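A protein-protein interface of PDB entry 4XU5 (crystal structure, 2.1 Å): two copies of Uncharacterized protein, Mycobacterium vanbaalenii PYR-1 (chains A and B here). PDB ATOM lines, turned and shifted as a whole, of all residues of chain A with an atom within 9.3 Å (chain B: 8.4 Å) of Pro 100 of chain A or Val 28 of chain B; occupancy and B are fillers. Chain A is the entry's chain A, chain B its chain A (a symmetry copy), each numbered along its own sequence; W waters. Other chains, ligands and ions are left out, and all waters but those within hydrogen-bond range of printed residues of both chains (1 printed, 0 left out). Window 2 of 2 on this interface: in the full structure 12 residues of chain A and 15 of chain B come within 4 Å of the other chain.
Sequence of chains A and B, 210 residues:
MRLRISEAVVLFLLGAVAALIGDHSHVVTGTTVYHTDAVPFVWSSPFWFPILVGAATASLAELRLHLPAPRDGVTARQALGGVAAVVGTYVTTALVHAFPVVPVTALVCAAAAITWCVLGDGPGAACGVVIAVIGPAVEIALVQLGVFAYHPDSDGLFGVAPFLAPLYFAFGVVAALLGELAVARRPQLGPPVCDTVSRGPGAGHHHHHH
OG of Ser 25 of chain B sits at hydrogen-bond distance from O of Ile 21 of chain B, at 3.0 Å. The indole nitrogen of Trp 43 of chain B sits at hydrogen-bond distance from a ring nitrogen (ND1) of His 24 of chain B (3.3 Å). A ring nitrogen (ND1) of His 24 of chain B sits at hydrogen-bond distance from the side-chain hydroxyl of Ser 44 of chain B (2.7 Å). O of Ser 25 of chain B sits at hydrogen-bond distance from OG1 of Thr 29 of chain B (2.7 Å). O of His 26 of chain B is in hydrogen-bond range of OG1 of Thr 29 of chain B (3.3 Å). The backbone carbonyl oxygen (O) of Thr 29 of chain B lies close to a ring nitrogen (NE2) of His 97 of chain B, 3.5 Å away.
Phe 99 of chain A touches Leu 95 of chain B (CE1 to O, 3.4 Å). Val 102 of chain A touches Ile 21 of chain B (CG1 to CG2, 3.995 Å). Val 102 of chain A touches His 24 of chain B (CB to CD2, 3.6 Å). Val 102 of chain A touches Ser 25 of chain B. Val 102 of chain A touches Trp 43 of chain B (CG2 to CZ2, 3.8 Å). Ser 25 of chain B touches Pro 103 of chain A. Pro 103 of chain A touches Leu 95 of chain B. Val 91 of chain B touches Ala 106 of chain A (CG1 to CB, 3.9 Å). Leu 107 of chain A touches Val 91 of chain B (N to CG2, 3.8 Å). CD2 of Leu 107 of chain A touches CD1 of Leu 95 of chain B, at 3.9 Å.
Pro 100 of chain A touches just these residues of chain B: Val 28 (3.6 Å) and Thr 29 (3.97 Å). Val 28 of chain B touches one residue of chain A. No residue of chain A comes within 4 Å of Val 27 of chain B. Of the printed residues of chain A, Thr 29 of chain B touches Pro 100. Printed residues of chain B within 4 Å of Leu 107 of chain A: Val 91 (3.8 Å) and Leu 95 (3.9 Å). Of the printed residues of chain A, Ile 21 of chain B touches Val 102 (3.995 Å). Ser 44 of chain B touches none of the printed residues of chain A. The nearest residue of chain B that does not touch Pro 100 of chain A is Leu 95 of chain B (5.0 Å). The nearest printed residue of chain A that does not touch Ile 21 of chain B is Ala 106 of chain A (4.1 Å).
Hydrophobic or aromatic side chains of chain A that line the printed part of chain B: Phe 99, Pro 100, Val 102, Pro 103, Ala 106 and Leu 107. Among the printed residues, 13 pairs touch across the chains. Among the printed residues, no Asp or Glu carboxylate lies within 4 Å of a Lys or Arg side-chain nitrogen of the other chain.
Position printed for both chains: 97. Of the 13 pairs that touch across the chains among the printed residues, none has its exchanged pair printed and touching as well.
Water W1 bridges NE2 of His 24 of chain B and N of Val 102 of chain A.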
ATOM      1  N   VAL A  96      17.006 -11.311 -10.935  1.00  0.00           N
ATOM      2  CA  VAL A  96      16.037 -11.338 -12.027  1.00  0.00           C
ATOM      3  C   VAL A  96      15.888 -10.019 -12.789  1.00  0.00           C
ATOM      4  O   VAL A  96      15.025  -9.902 -13.655  1.00  0.00           O
ATOM      5  CB  VAL A  96      14.633 -11.776 -11.538  1.00  0.00           C
ATOM      6  CG1 VAL A  96      14.690 -13.175 -10.918  1.00  0.00           C
ATOM      7  CG2 VAL A  96      14.037 -10.739 -10.548  1.00  0.00           C
ATOM      8  N   HIS A  97      16.730  -9.040 -12.461  1.00  0.00           N
ATOM      9  CA  HIS A  97      16.616  -7.682 -12.990  1.00  0.00           C
ATOM     10  C   HIS A  97      16.609  -7.583 -14.516  1.00  0.00           C
ATOM     11  O   HIS A  97      16.070  -6.623 -15.073  1.00  0.00           O
ATOM     12  CB  HIS A  97      17.769  -6.822 -12.464  1.00  0.00           C
ATOM     13  CG  HIS A  97      19.069  -7.078 -13.159  1.00  0.00           C
ATOM     14  ND1 HIS A  97      19.943  -8.065 -12.758  1.00  0.00           N
ATOM     15  CD2 HIS A  97      19.626  -6.499 -14.250  1.00  0.00           C
ATOM     16  CE1 HIS A  97      20.989  -8.075 -13.565  1.00  0.00           C
ATOM     17  NE2 HIS A  97      20.826  -7.129 -14.475  1.00  0.00           N
ATOM     18  N   ALA A  98      17.217  -8.557 -15.195  1.00  0.00           N
ATOM     19  CA  ALA A  98      17.304  -8.502 -16.655  1.00  0.00           C
ATOM     20  C   ALA A  98      16.100  -9.138 -17.338  1.00  0.00           C
ATOM     21  O   ALA A  98      16.013  -9.150 -18.563  1.00  0.00           O
ATOM     22  CB  ALA A  98      18.608  -9.150 -17.153  1.00  0.00           C
ATOM     23  N   PHE A  99      15.173  -9.667 -16.555  1.00  0.00           N
ATOM     24  CA  PHE A  99      14.003 -10.330 -17.118  1.00  0.00           C
ATOM     25  C   PHE A  99      12.966  -9.275 -17.445  1.00  0.00           C
ATOM     26  O   PHE A  99      13.109  -8.128 -17.018  1.00  0.00           O
ATOM     27  CB  PHE A  99      13.463 -11.381 -16.137  1.00  0.00           C
ATOM     28  CG  PHE A  99      14.223 -12.684 -16.155  1.00  0.00           C
ATOM     29  CD1 PHE A  99      13.873 -13.698 -17.051  1.00  0.00           C
ATOM     30  CD2 PHE A  99      15.280 -12.901 -15.281  1.00  0.00           C
ATOM     31  CE1 PHE A  99      14.570 -14.902 -17.074  1.00  0.00           C
ATOM     32  CE2 PHE A  99      15.988 -14.101 -15.292  1.00  0.00           C
ATOM     33  CZ  PHE A  99      15.631 -15.107 -16.193  1.00  0.00           C
ATOM     34  N   PRO A 100      11.926  -9.637 -18.219  1.00  0.00           N
ATOM     35  CA  PRO A 100      10.866  -8.670 -18.535  1.00  0.00           C
ATOM     36  C   PRO A 100      10.211  -8.039 -17.307  1.00  0.00           C
ATOM     37  O   PRO A 100       9.986  -8.708 -16.279  1.00  0.00           O
ATOM     38  CB  PRO A 100       9.865  -9.514 -19.328  1.00  0.00           C
ATOM     39  CG  PRO A 100      10.769 -10.476 -20.085  1.00  0.00           C
ATOM     40  CD  PRO A 100      11.793 -10.864 -19.032  1.00  0.00           C
ATOM     41  N   VAL A 101       9.886  -6.756 -17.449  1.00  0.00           N
ATOM     42  CA  VAL A 101       9.468  -5.907 -16.337  1.00  0.00           C
ATOM     43  C   VAL A 101       8.180  -6.360 -15.635  1.00  0.00           C
ATOM     44  O   VAL A 101       8.058  -6.231 -14.414  1.00  0.00           O
ATOM     45  CB  VAL A 101       9.353  -4.426 -16.801  1.00  0.00           C
ATOM     46  CG1 VAL A 101       8.318  -4.280 -17.917  1.00  0.00           C
ATOM     47  CG2 VAL A 101       9.037  -3.506 -15.631  1.00  0.00           C
ATOM     48  N   VAL A 102       7.219  -6.887 -16.390  1.00  0.00           N
ATOM     49  CA  VAL A 102       5.957  -7.281 -15.773  1.00  0.00           C
ATOM     50  C   VAL A 102       6.109  -8.461 -14.791  1.00  0.00           C
ATOM     51  O   VAL A 102       5.727  -8.326 -13.633  1.00  0.00           O
ATOM     52  CB  VAL A 102       4.793  -7.496 -16.808  1.00  0.00           C
ATOM     53  CG1 VAL A 102       3.604  -8.204 -16.150  1.00  0.00           C
ATOM     54  CG2 VAL A 102       4.352  -6.161 -17.403  1.00  0.00           C
ATOM     55  N   PRO A 103       6.670  -9.602 -15.241  1.00  0.00           N
ATOM     56  CA  PRO A 103       6.787 -10.702 -14.271  1.00  0.00           C
ATOM     57  C   PRO A 103       7.713 -10.346 -13.116  1.00  0.00           C
ATOM     58  O   PRO A 103       7.455 -10.776 -12.002  1.00  0.00           O
ATOM     59  CB  PRO A 103       7.380 -11.853 -15.096  1.00  0.00           C
ATOM     60  CG  PRO A 103       7.993 -11.177 -16.334  1.00  0.00           C
ATOM     61  CD  PRO A 103       7.105 -10.008 -16.598  1.00  0.00           C
ATOM     62  N   VAL A 104       8.763  -9.570 -13.380  1.00  0.00           N
ATOM     63  CA  VAL A 104       9.691  -9.175 -12.325  1.00  0.00           C
ATOM     64  C   VAL A 104       9.005  -8.316 -11.264  1.00  0.00           C
ATOM     65  O   VAL A 104       9.102  -8.591 -10.068  1.00  0.00           O
ATOM     66  CB  VAL A 104      10.922  -8.413 -12.888  1.00  0.00           C
ATOM     67  CG1 VAL A 104      11.735  -7.788 -11.748  1.00  0.00           C
ATOM     68  CG2 VAL A 104      11.784  -9.342 -13.722  1.00  0.00           C
ATOM     69  N   THR A 105       8.327  -7.266 -11.710  1.00  0.00           N
ATOM     70  CA  THR A 105       7.656  -6.356 -10.789  1.00  0.00           C
ATOM     71  C   THR A 105       6.521  -7.059 -10.028  1.00  0.00           C
ATOM     72  O   THR A 105       6.358  -6.864  -8.820  1.00  0.00           O
ATOM     73  CB  THR A 105       7.115  -5.120 -11.524  1.00  0.00           C
ATOM     74  OG1 THR A 105       8.180  -4.509 -12.273  1.00  0.00           O
ATOM     75  CG2 THR A 105       6.543  -4.116 -10.525  1.00  0.00           C
ATOM     76  N   ALA A 106       5.760  -7.883 -10.746  1.00  0.00           N
ATOM     77  CA  ALA A 106       4.699  -8.685 -10.144  1.00  0.00           C
ATOM     78  C   ALA A 106       5.252  -9.636  -9.086  1.00  0.00           C
ATOM     79  O   ALA A 106       4.634  -9.846  -8.030  1.00  0.00           O
ATOM     80  CB  ALA A 106       3.951  -9.472 -11.226  1.00  0.00           C
ATOM     81  N   LEU A 107       6.413 -10.224  -9.364  1.00  0.00           N
ATOM     82  CA  LEU A 107       7.013 -11.141  -8.396  1.00  0.00           C
ATOM     83  C   LEU A 107       7.341 -10.398  -7.103  1.00  0.00           C
ATOM     84  O   LEU A 107       7.096 -10.886  -6.005  1.00  0.00           O
ATOM     85  CB  LEU A 107       8.270 -11.799  -8.966  1.00  0.00           C
ATOM     86  CG  LEU A 107       9.051 -12.666  -7.968  1.00  0.00           C
ATOM     87  CD1 LEU A 107       8.186 -13.792  -7.401  1.00  0.00           C
ATOM     88  CD2 LEU A 107      10.305 -13.223  -8.627  1.00  0.00           C
ATOM     89  N   VAL A 108       7.893  -9.203  -7.240  1.00  0.00           N
ATOM     90  CA  VAL A 108       8.290  -8.448  -6.062  1.00  0.00           C
ATOM     91  C   VAL A 108       7.069  -7.918  -5.295  1.00  0.00           C
ATOM     92  O   VAL A 108       7.080  -7.870  -4.060  1.00  0.00           O
ATOM     93  CB  VAL A 108       9.279  -7.318  -6.417  1.00  0.00           C
ATOM     94  CG1 VAL A 108       9.630  -6.494  -5.168  1.00  0.00           C
ATOM     95  CG2 VAL A 108      10.547  -7.915  -7.063  1.00  0.00           C
ATOM     96  N   HIS A 151      20.394  -0.705 -14.898  1.00  0.00           N
ATOM     97  CA  HIS A 151      20.402  -1.477 -16.126  1.00  0.00           C
ATOM     98  C   HIS A 151      19.216  -1.065 -17.004  1.00  0.00           C
ATOM     99  O   HIS A 151      18.138  -0.799 -16.494  1.00  0.00           O
ATOM    100  CB  HIS A 151      20.296  -2.954 -15.761  1.00  0.00           C
ATOM    101  CG  HIS A 151      20.449  -3.885 -16.924  1.00  0.00           C
ATOM    102  ND1 HIS A 151      19.426  -4.149 -17.806  1.00  0.00           N
ATOM    103  CD2 HIS A 151      21.500  -4.639 -17.328  1.00  0.00           C
ATOM    104  CE1 HIS A 151      19.843  -5.012 -18.714  1.00  0.00           C
ATOM    105  NE2 HIS A 151      21.097  -5.323 -18.448  1.00  0.00           N
ATOM    106  N   ASP A 153      17.214  -2.662 -18.863  1.00  0.00           N
ATOM    107  CA  ASP A 153      16.028  -3.505 -18.730  1.00  0.00           C
ATOM    108  C   ASP A 153      15.405  -3.371 -17.352  1.00  0.00           C
ATOM    109  O   ASP A 153      14.497  -4.118 -16.996  1.00  0.00           O
ATOM    110  CB  ASP A 153      16.366  -4.972 -19.009  1.00  0.00           C
ATOM    111  CG  ASP A 153      16.852  -5.193 -20.434  1.00  0.00           C
ATOM    112  OD1 ASP A 153      16.352  -4.497 -21.348  1.00  0.00           O
ATOM    113  OD2 ASP A 153      17.741  -6.056 -20.641  1.00  0.00           O
ATOM    114  N   SER A 154      15.868  -2.391 -16.585  1.00  0.00           N
ATOM    115  CA  SER A 154      15.487  -2.297 -15.184  1.00  0.00           C
ATOM    116  C   SER A 154      15.379  -0.838 -14.737  1.00  0.00           C
ATOM    117  O   SER A 154      15.659  -0.516 -13.581  1.00  0.00           O
ATOM    118  CB  SER A 154      16.532  -3.033 -14.345  1.00  0.00           C
ATOM    119  OG  SER A 154      15.957  -3.616 -13.199  1.00  0.00           O
ATOM    120  N   PRO A 162      11.040  -0.323 -11.486  1.00  0.00           N
ATOM    121  CA  PRO A 162       9.690  -0.342 -10.898  1.00  0.00           C
ATOM    122  C   PRO A 162       9.599  -1.235  -9.658  1.00  0.00           C
ATOM    123  O   PRO A 162       8.761  -0.961  -8.805  1.00  0.00           O
ATOM    124  CB  PRO A 162       8.810  -0.876 -12.035  1.00  0.00           C
ATOM    125  CG  PRO A 162       9.553  -0.494 -13.298  1.00  0.00           C
ATOM    126  CD  PRO A 162      11.032  -0.568 -12.940  1.00  0.00           C
ATOM    127  N   PHE A 163      10.456  -2.252  -9.538  1.00  0.00           N
ATOM    128  CA  PHE A 163      10.413  -3.129  -8.357  1.00  0.00           C
ATOM    129  C   PHE A 163      10.770  -2.400  -7.056  1.00  0.00           C
ATOM    130  O   PHE A 163      10.504  -2.896  -5.957  1.00  0.00           O
ATOM    131  CB  PHE A 163      11.234  -4.438  -8.538  1.00  0.00           C
ATOM    132  CG  PHE A 163      12.740  -4.236  -8.703  1.00  0.00           C
ATOM    133  CD1 PHE A 163      13.518  -3.689  -7.681  1.00  0.00           C
ATOM    134  CD2 PHE A 163      13.378  -4.645  -9.876  1.00  0.00           C
ATOM    135  CE1 PHE A 163      14.911  -3.520  -7.836  1.00  0.00           C
ATOM    136  CE2 PHE A 163      14.773  -4.496 -10.042  1.00  0.00           C
ATOM    137  CZ  PHE A 163      15.538  -3.928  -9.018  1.00  0.00           C
ATOM    138  N   ILE B  21      -2.000 -10.795 -16.332  1.00  0.00           N
ATOM    139  CA  ILE B  21      -0.636 -10.550 -15.882  1.00  0.00           C
ATOM    140  C   ILE B  21       0.242 -11.779 -16.091  1.00  0.00           C
ATOM    141  O   ILE B  21       1.340 -11.681 -16.659  1.00  0.00           O
ATOM    142  CB  ILE B  21      -0.589 -10.114 -14.401  1.00  0.00           C
ATOM    143  CG1 ILE B  21      -1.284  -8.760 -14.212  1.00  0.00           C
ATOM    144  CG2 ILE B  21       0.855 -10.046 -13.911  1.00  0.00           C
ATOM    145  CD1 ILE B  21      -1.570  -8.414 -12.722  1.00  0.00           C
ATOM    146  N   GLY B  22      -0.241 -12.936 -15.636  1.00  0.00           N
ATOM    147  CA  GLY B  22       0.498 -14.180 -15.756  1.00  0.00           C
ATOM    148  C   GLY B  22       0.713 -14.613 -17.204  1.00  0.00           C
ATOM    149  O   GLY B  22       1.801 -15.075 -17.582  1.00  0.00           O
ATOM    150  N   ASP B  23      -0.329 -14.480 -18.018  1.00  0.00           N
ATOM    151  CA  ASP B  23      -0.248 -14.912 -19.417  1.00  0.00           C
ATOM    152  C   ASP B  23       0.666 -13.981 -20.196  1.00  0.00           C
ATOM    153  O   ASP B  23       1.453 -14.433 -21.034  1.00  0.00           O
ATOM    154  CB  ASP B  23      -1.642 -14.957 -20.057  1.00  0.00           C
ATOM    155  CG  ASP B  23      -1.677 -15.792 -21.334  1.00  0.00           C
ATOM    156  OD1 ASP B  23      -1.011 -16.846 -21.384  1.00  0.00           O
ATOM    157  OD2 ASP B  23      -2.387 -15.391 -22.283  1.00  0.00           O
ATOM    158  N   HIS B  24       0.578 -12.678 -19.918  1.00  0.00           N
ATOM    159  CA  HIS B  24       1.531 -11.745 -20.521  1.00  0.00           C
ATOM    160  C   HIS B  24       2.978 -12.133 -20.187  1.00  0.00           C
ATOM    161  O   HIS B  24       3.867 -12.095 -21.052  1.00  0.00           O
ATOM    162  CB  HIS B  24       1.287 -10.303 -20.082  1.00  0.00           C
ATOM    163  CG  HIS B  24       2.380  -9.377 -20.504  1.00  0.00           C
ATOM    164  ND1 HIS B  24       2.445  -8.827 -21.769  1.00  0.00           N
ATOM    165  CD2 HIS B  24       3.495  -8.959 -19.856  1.00  0.00           C
ATOM    166  CE1 HIS B  24       3.536  -8.084 -21.869  1.00  0.00           C
ATOM    167  NE2 HIS B  24       4.189  -8.147 -20.721  1.00  0.00           N
ATOM    168  N   SER B  25       3.206 -12.508 -18.927  1.00  0.00           N
ATOM    169  CA  SER B  25       4.532 -12.946 -18.497  1.00  0.00           C
ATOM    170  C   SER B  25       5.018 -14.158 -19.300  1.00  0.00           C
ATOM    171  O   SER B  25       6.167 -14.195 -19.736  1.00  0.00           O
ATOM    172  CB  SER B  25       4.552 -13.231 -16.995  1.00  0.00           C
ATOM    173  OG  SER B  25       4.263 -12.054 -16.260  1.00  0.00           O
ATOM    174  N   HIS B  26       4.138 -15.128 -19.519  1.00  0.00           N
ATOM    175  CA  HIS B  26       4.468 -16.292 -20.342  1.00  0.00           C
ATOM    176  C   HIS B  26       4.812 -15.934 -21.803  1.00  0.00           C
ATOM    177  O   HIS B  26       5.740 -16.481 -22.399  1.00  0.00           O
ATOM    178  CB  HIS B  26       3.311 -17.298 -20.322  1.00  0.00           C
ATOM    179  CG  HIS B  26       3.328 -18.212 -19.139  1.00  0.00           C
ATOM    180  ND1 HIS B  26       2.355 -19.161 -18.919  1.00  0.00           N
ATOM    181  CD2 HIS B  26       4.209 -18.329 -18.117  1.00  0.00           C
ATOM    182  CE1 HIS B  26       2.629 -19.819 -17.807  1.00  0.00           C
ATOM    183  NE2 HIS B  26       3.753 -19.338 -17.304  1.00  0.00           N
ATOM    184  N   VAL B  27       4.035 -15.032 -22.385  1.00  0.00           N
ATOM    185  CA  VAL B  27       4.269 -14.638 -23.775  1.00  0.00           C
ATOM    186  C   VAL B  27       5.591 -13.881 -23.918  1.00  0.00           C
ATOM    187  O   VAL B  27       6.410 -14.209 -24.781  1.00  0.00           O
ATOM    188  CB  VAL B  27       3.088 -13.797 -24.332  1.00  0.00           C
ATOM    189  CG1 VAL B  27       3.444 -13.188 -25.687  1.00  0.00           C
ATOM    190  CG2 VAL B  27       1.810 -14.657 -24.439  1.00  0.00           C
ATOM    191  N   VAL B  28       5.801 -12.889 -23.056  1.00  0.00           N
ATOM    192  CA  VAL B  28       6.955 -11.999 -23.170  1.00  0.00           C
ATOM    193  C   VAL B  28       8.279 -12.692 -22.835  1.00  0.00           C
ATOM    194  O   VAL B  28       9.325 -12.272 -23.288  1.00  0.00           O
ATOM    195  CB  VAL B  28       6.762 -10.705 -22.329  1.00  0.00           C
ATOM    196  CG1 VAL B  28       6.948 -10.972 -20.811  1.00  0.00           C
ATOM    197  CG2 VAL B  28       7.686  -9.609 -22.819  1.00  0.00           C
ATOM    198  N   THR B  29       8.225 -13.776 -22.061  1.00  0.00           N
ATOM    199  CA  THR B  29       9.425 -14.561 -21.773  1.00  0.00           C
ATOM    200  C   THR B  29       9.626 -15.690 -22.785  1.00  0.00           C
ATOM    201  O   THR B  29      10.616 -16.410 -22.718  1.00  0.00           O
ATOM    202  CB  THR B  29       9.370 -15.198 -20.362  1.00  0.00           C
ATOM    203  OG1 THR B  29       8.165 -15.963 -20.244  1.00  0.00           O
ATOM    204  CG2 THR B  29       9.412 -14.118 -19.261  1.00  0.00           C
ATOM    205  N   GLY B  30       8.682 -15.853 -23.706  1.00  0.00           N
ATOM    206  CA  GLY B  30       8.722 -16.965 -24.642  1.00  0.00           C
ATOM    207  C   GLY B  30       8.341 -18.312 -24.041  1.00  0.00           C
ATOM    208  O   GLY B  30       8.662 -19.364 -24.595  1.00  0.00           O
ATOM    209  N   THR B  31       7.664 -18.289 -22.896  1.00  0.00           N
ATOM    210  CA  THR B  31       7.168 -19.526 -22.301  1.00  0.00           C
ATOM    211  C   THR B  31       6.128 -20.140 -23.231  1.00  0.00           C
ATOM    212  O   THR B  31       6.061 -21.358 -23.376  1.00  0.00           O
ATOM    213  CB  THR B  31       6.526 -19.273 -20.913  1.00  0.00           C
ATOM    214  OG1 THR B  31       7.497 -18.680 -20.035  1.00  0.00           O
ATOM    215  CG2 THR B  31       5.983 -20.587 -20.301  1.00  0.00           C
ATOM    216  N   THR B  32       5.311 -19.284 -23.844  1.00  0.00           N
ATOM    217  CA  THR B  32       4.265 -19.708 -24.771  1.00  0.00           C
ATOM    218  C   THR B  32       4.170 -18.739 -25.954  1.00  0.00           C
ATOM    219  O   THR B  32       4.611 -17.595 -25.869  1.00  0.00           O
ATOM    220  CB  THR B  32       2.877 -19.745 -24.089  1.00  0.00           C
ATOM    221  OG1 THR B  32       2.533 -18.437 -23.627  1.00  0.00           O
ATOM    222  CG2 THR B  32       2.887 -20.656 -22.901  1.00  0.00           C
ATOM    223  N   VAL B  33       3.593 -19.209 -27.057  1.00  0.00           N
ATOM    224  CA  VAL B  33       3.315 -18.361 -28.212  1.00  0.00           C
ATOM    225  C   VAL B  33       1.916 -18.691 -28.694  1.00  0.00           C
ATOM    226  O   VAL B  33       1.561 -19.860 -28.819  1.00  0.00           O
ATOM    227  CB  VAL B  33       4.296 -18.609 -29.398  1.00  0.00           C
ATOM    228  CG1 VAL B  33       3.925 -17.738 -30.587  1.00  0.00           C
ATOM    229  CG2 VAL B  33       5.743 -18.352 -28.999  1.00  0.00           C
ATOM    230  N   TRP B  43      -4.549  -7.221 -24.076  1.00  0.00           N
ATOM    231  CA  TRP B  43      -3.112  -7.234 -23.790  1.00  0.00           C
ATOM    232  C   TRP B  43      -2.433  -8.320 -24.640  1.00  0.00           C
ATOM    233  O   TRP B  43      -2.551  -8.303 -25.862  1.00  0.00           O
ATOM    234  CB  TRP B  43      -2.870  -7.438 -22.289  1.00  0.00           C
ATOM    235  CG  TRP B  43      -1.529  -6.970 -21.803  1.00  0.00           C
ATOM    236  CD1 TRP B  43      -0.512  -6.447 -22.552  1.00  0.00           C
ATOM    237  CD2 TRP B  43      -1.059  -6.986 -20.449  1.00  0.00           C
ATOM    238  NE1 TRP B  43       0.556  -6.131 -21.746  1.00  0.00           N
ATOM    239  CE2 TRP B  43       0.243  -6.451 -20.450  1.00  0.00           C
ATOM    240  CE3 TRP B  43      -1.623  -7.395 -19.234  1.00  0.00           C
ATOM    241  CZ2 TRP B  43       0.998  -6.320 -19.284  1.00  0.00           C
ATOM    242  CZ3 TRP B  43      -0.867  -7.264 -18.074  1.00  0.00           C
ATOM    243  CH2 TRP B  43       0.427  -6.735 -18.111  1.00  0.00           C
ATOM    244  N   SER B  44      -1.762  -9.284 -24.009  1.00  0.00           N
ATOM    245  CA  SER B  44      -1.093 -10.343 -24.776  1.00  0.00           C
ATOM    246  C   SER B  44      -1.918 -11.628 -24.950  1.00  0.00           C
ATOM    247  O   SER B  44      -1.395 -12.642 -25.409  1.00  0.00           O
ATOM    248  CB  SER B  44       0.263 -10.691 -24.156  1.00  0.00           C
ATOM    249  OG  SER B  44       1.063  -9.533 -23.987  1.00  0.00           O
ATOM    250  N   VAL B  91       4.046 -15.978 -12.248  1.00  0.00           N
ATOM    251  CA  VAL B  91       5.085 -15.215 -12.938  1.00  0.00           C
ATOM    252  C   VAL B  91       6.438 -15.885 -12.801  1.00  0.00           C
ATOM    253  O   VAL B  91       7.283 -15.742 -13.671  1.00  0.00           O
ATOM    254  CB  VAL B  91       5.159 -13.707 -12.525  1.00  0.00           C
ATOM    255  CG1 VAL B  91       3.861 -12.970 -12.893  1.00  0.00           C
ATOM    256  CG2 VAL B  91       5.473 -13.543 -11.041  1.00  0.00           C
ATOM    257  N   ALA B  94       7.103 -18.219 -15.661  1.00  0.00           N
ATOM    258  CA  ALA B  94       7.604 -17.490 -16.831  1.00  0.00           C
ATOM    259  C   ALA B  94       9.108 -17.279 -16.724  1.00  0.00           C
ATOM    260  O   ALA B  94       9.838 -17.411 -17.706  1.00  0.00           O
ATOM    261  CB  ALA B  94       6.902 -16.137 -16.964  1.00  0.00           C
ATOM    262  N   LEU B  95       9.581 -16.929 -15.530  1.00  0.00           N
ATOM    263  CA  LEU B  95      11.006 -16.622 -15.378  1.00  0.00           C
ATOM    264  C   LEU B  95      11.912 -17.854 -15.492  1.00  0.00           C
ATOM    265  O   LEU B  95      13.042 -17.737 -15.939  1.00  0.00           O
ATOM    266  CB  LEU B  95      11.274 -15.892 -14.055  1.00  0.00           C
ATOM    267  CG  LEU B  95      10.535 -14.577 -13.794  1.00  0.00           C
ATOM    268  CD1 LEU B  95      10.842 -14.089 -12.377  1.00  0.00           C
ATOM    269  CD2 LEU B  95      10.876 -13.505 -14.838  1.00  0.00           C
ATOM    270  N   HIS B  97      11.005 -21.006 -16.948  1.00  0.00           N
ATOM    271  CA  HIS B  97      10.472 -21.989 -17.887  1.00  0.00           C
ATOM    272  C   HIS B  97      11.520 -22.686 -18.756  1.00  0.00           C
ATOM    273  O   HIS B  97      11.295 -23.806 -19.221  1.00  0.00           O
ATOM    274  CB  HIS B  97       9.455 -21.320 -18.816  1.00  0.00           C
ATOM    275  CG  HIS B  97      10.084 -20.499 -19.896  1.00  0.00           C
ATOM    276  ND1 HIS B  97      10.429 -19.176 -19.719  1.00  0.00           N
ATOM    277  CD2 HIS B  97      10.466 -20.822 -21.156  1.00  0.00           C
ATOM    278  CE1 HIS B  97      10.983 -18.716 -20.826  1.00  0.00           C
ATOM    279  NE2 HIS B  97      11.011 -19.694 -21.718  1.00  0.00           N
HETATM  280  O   HOH W   1       6.877  -7.279 -19.568  1.00  0.00           O
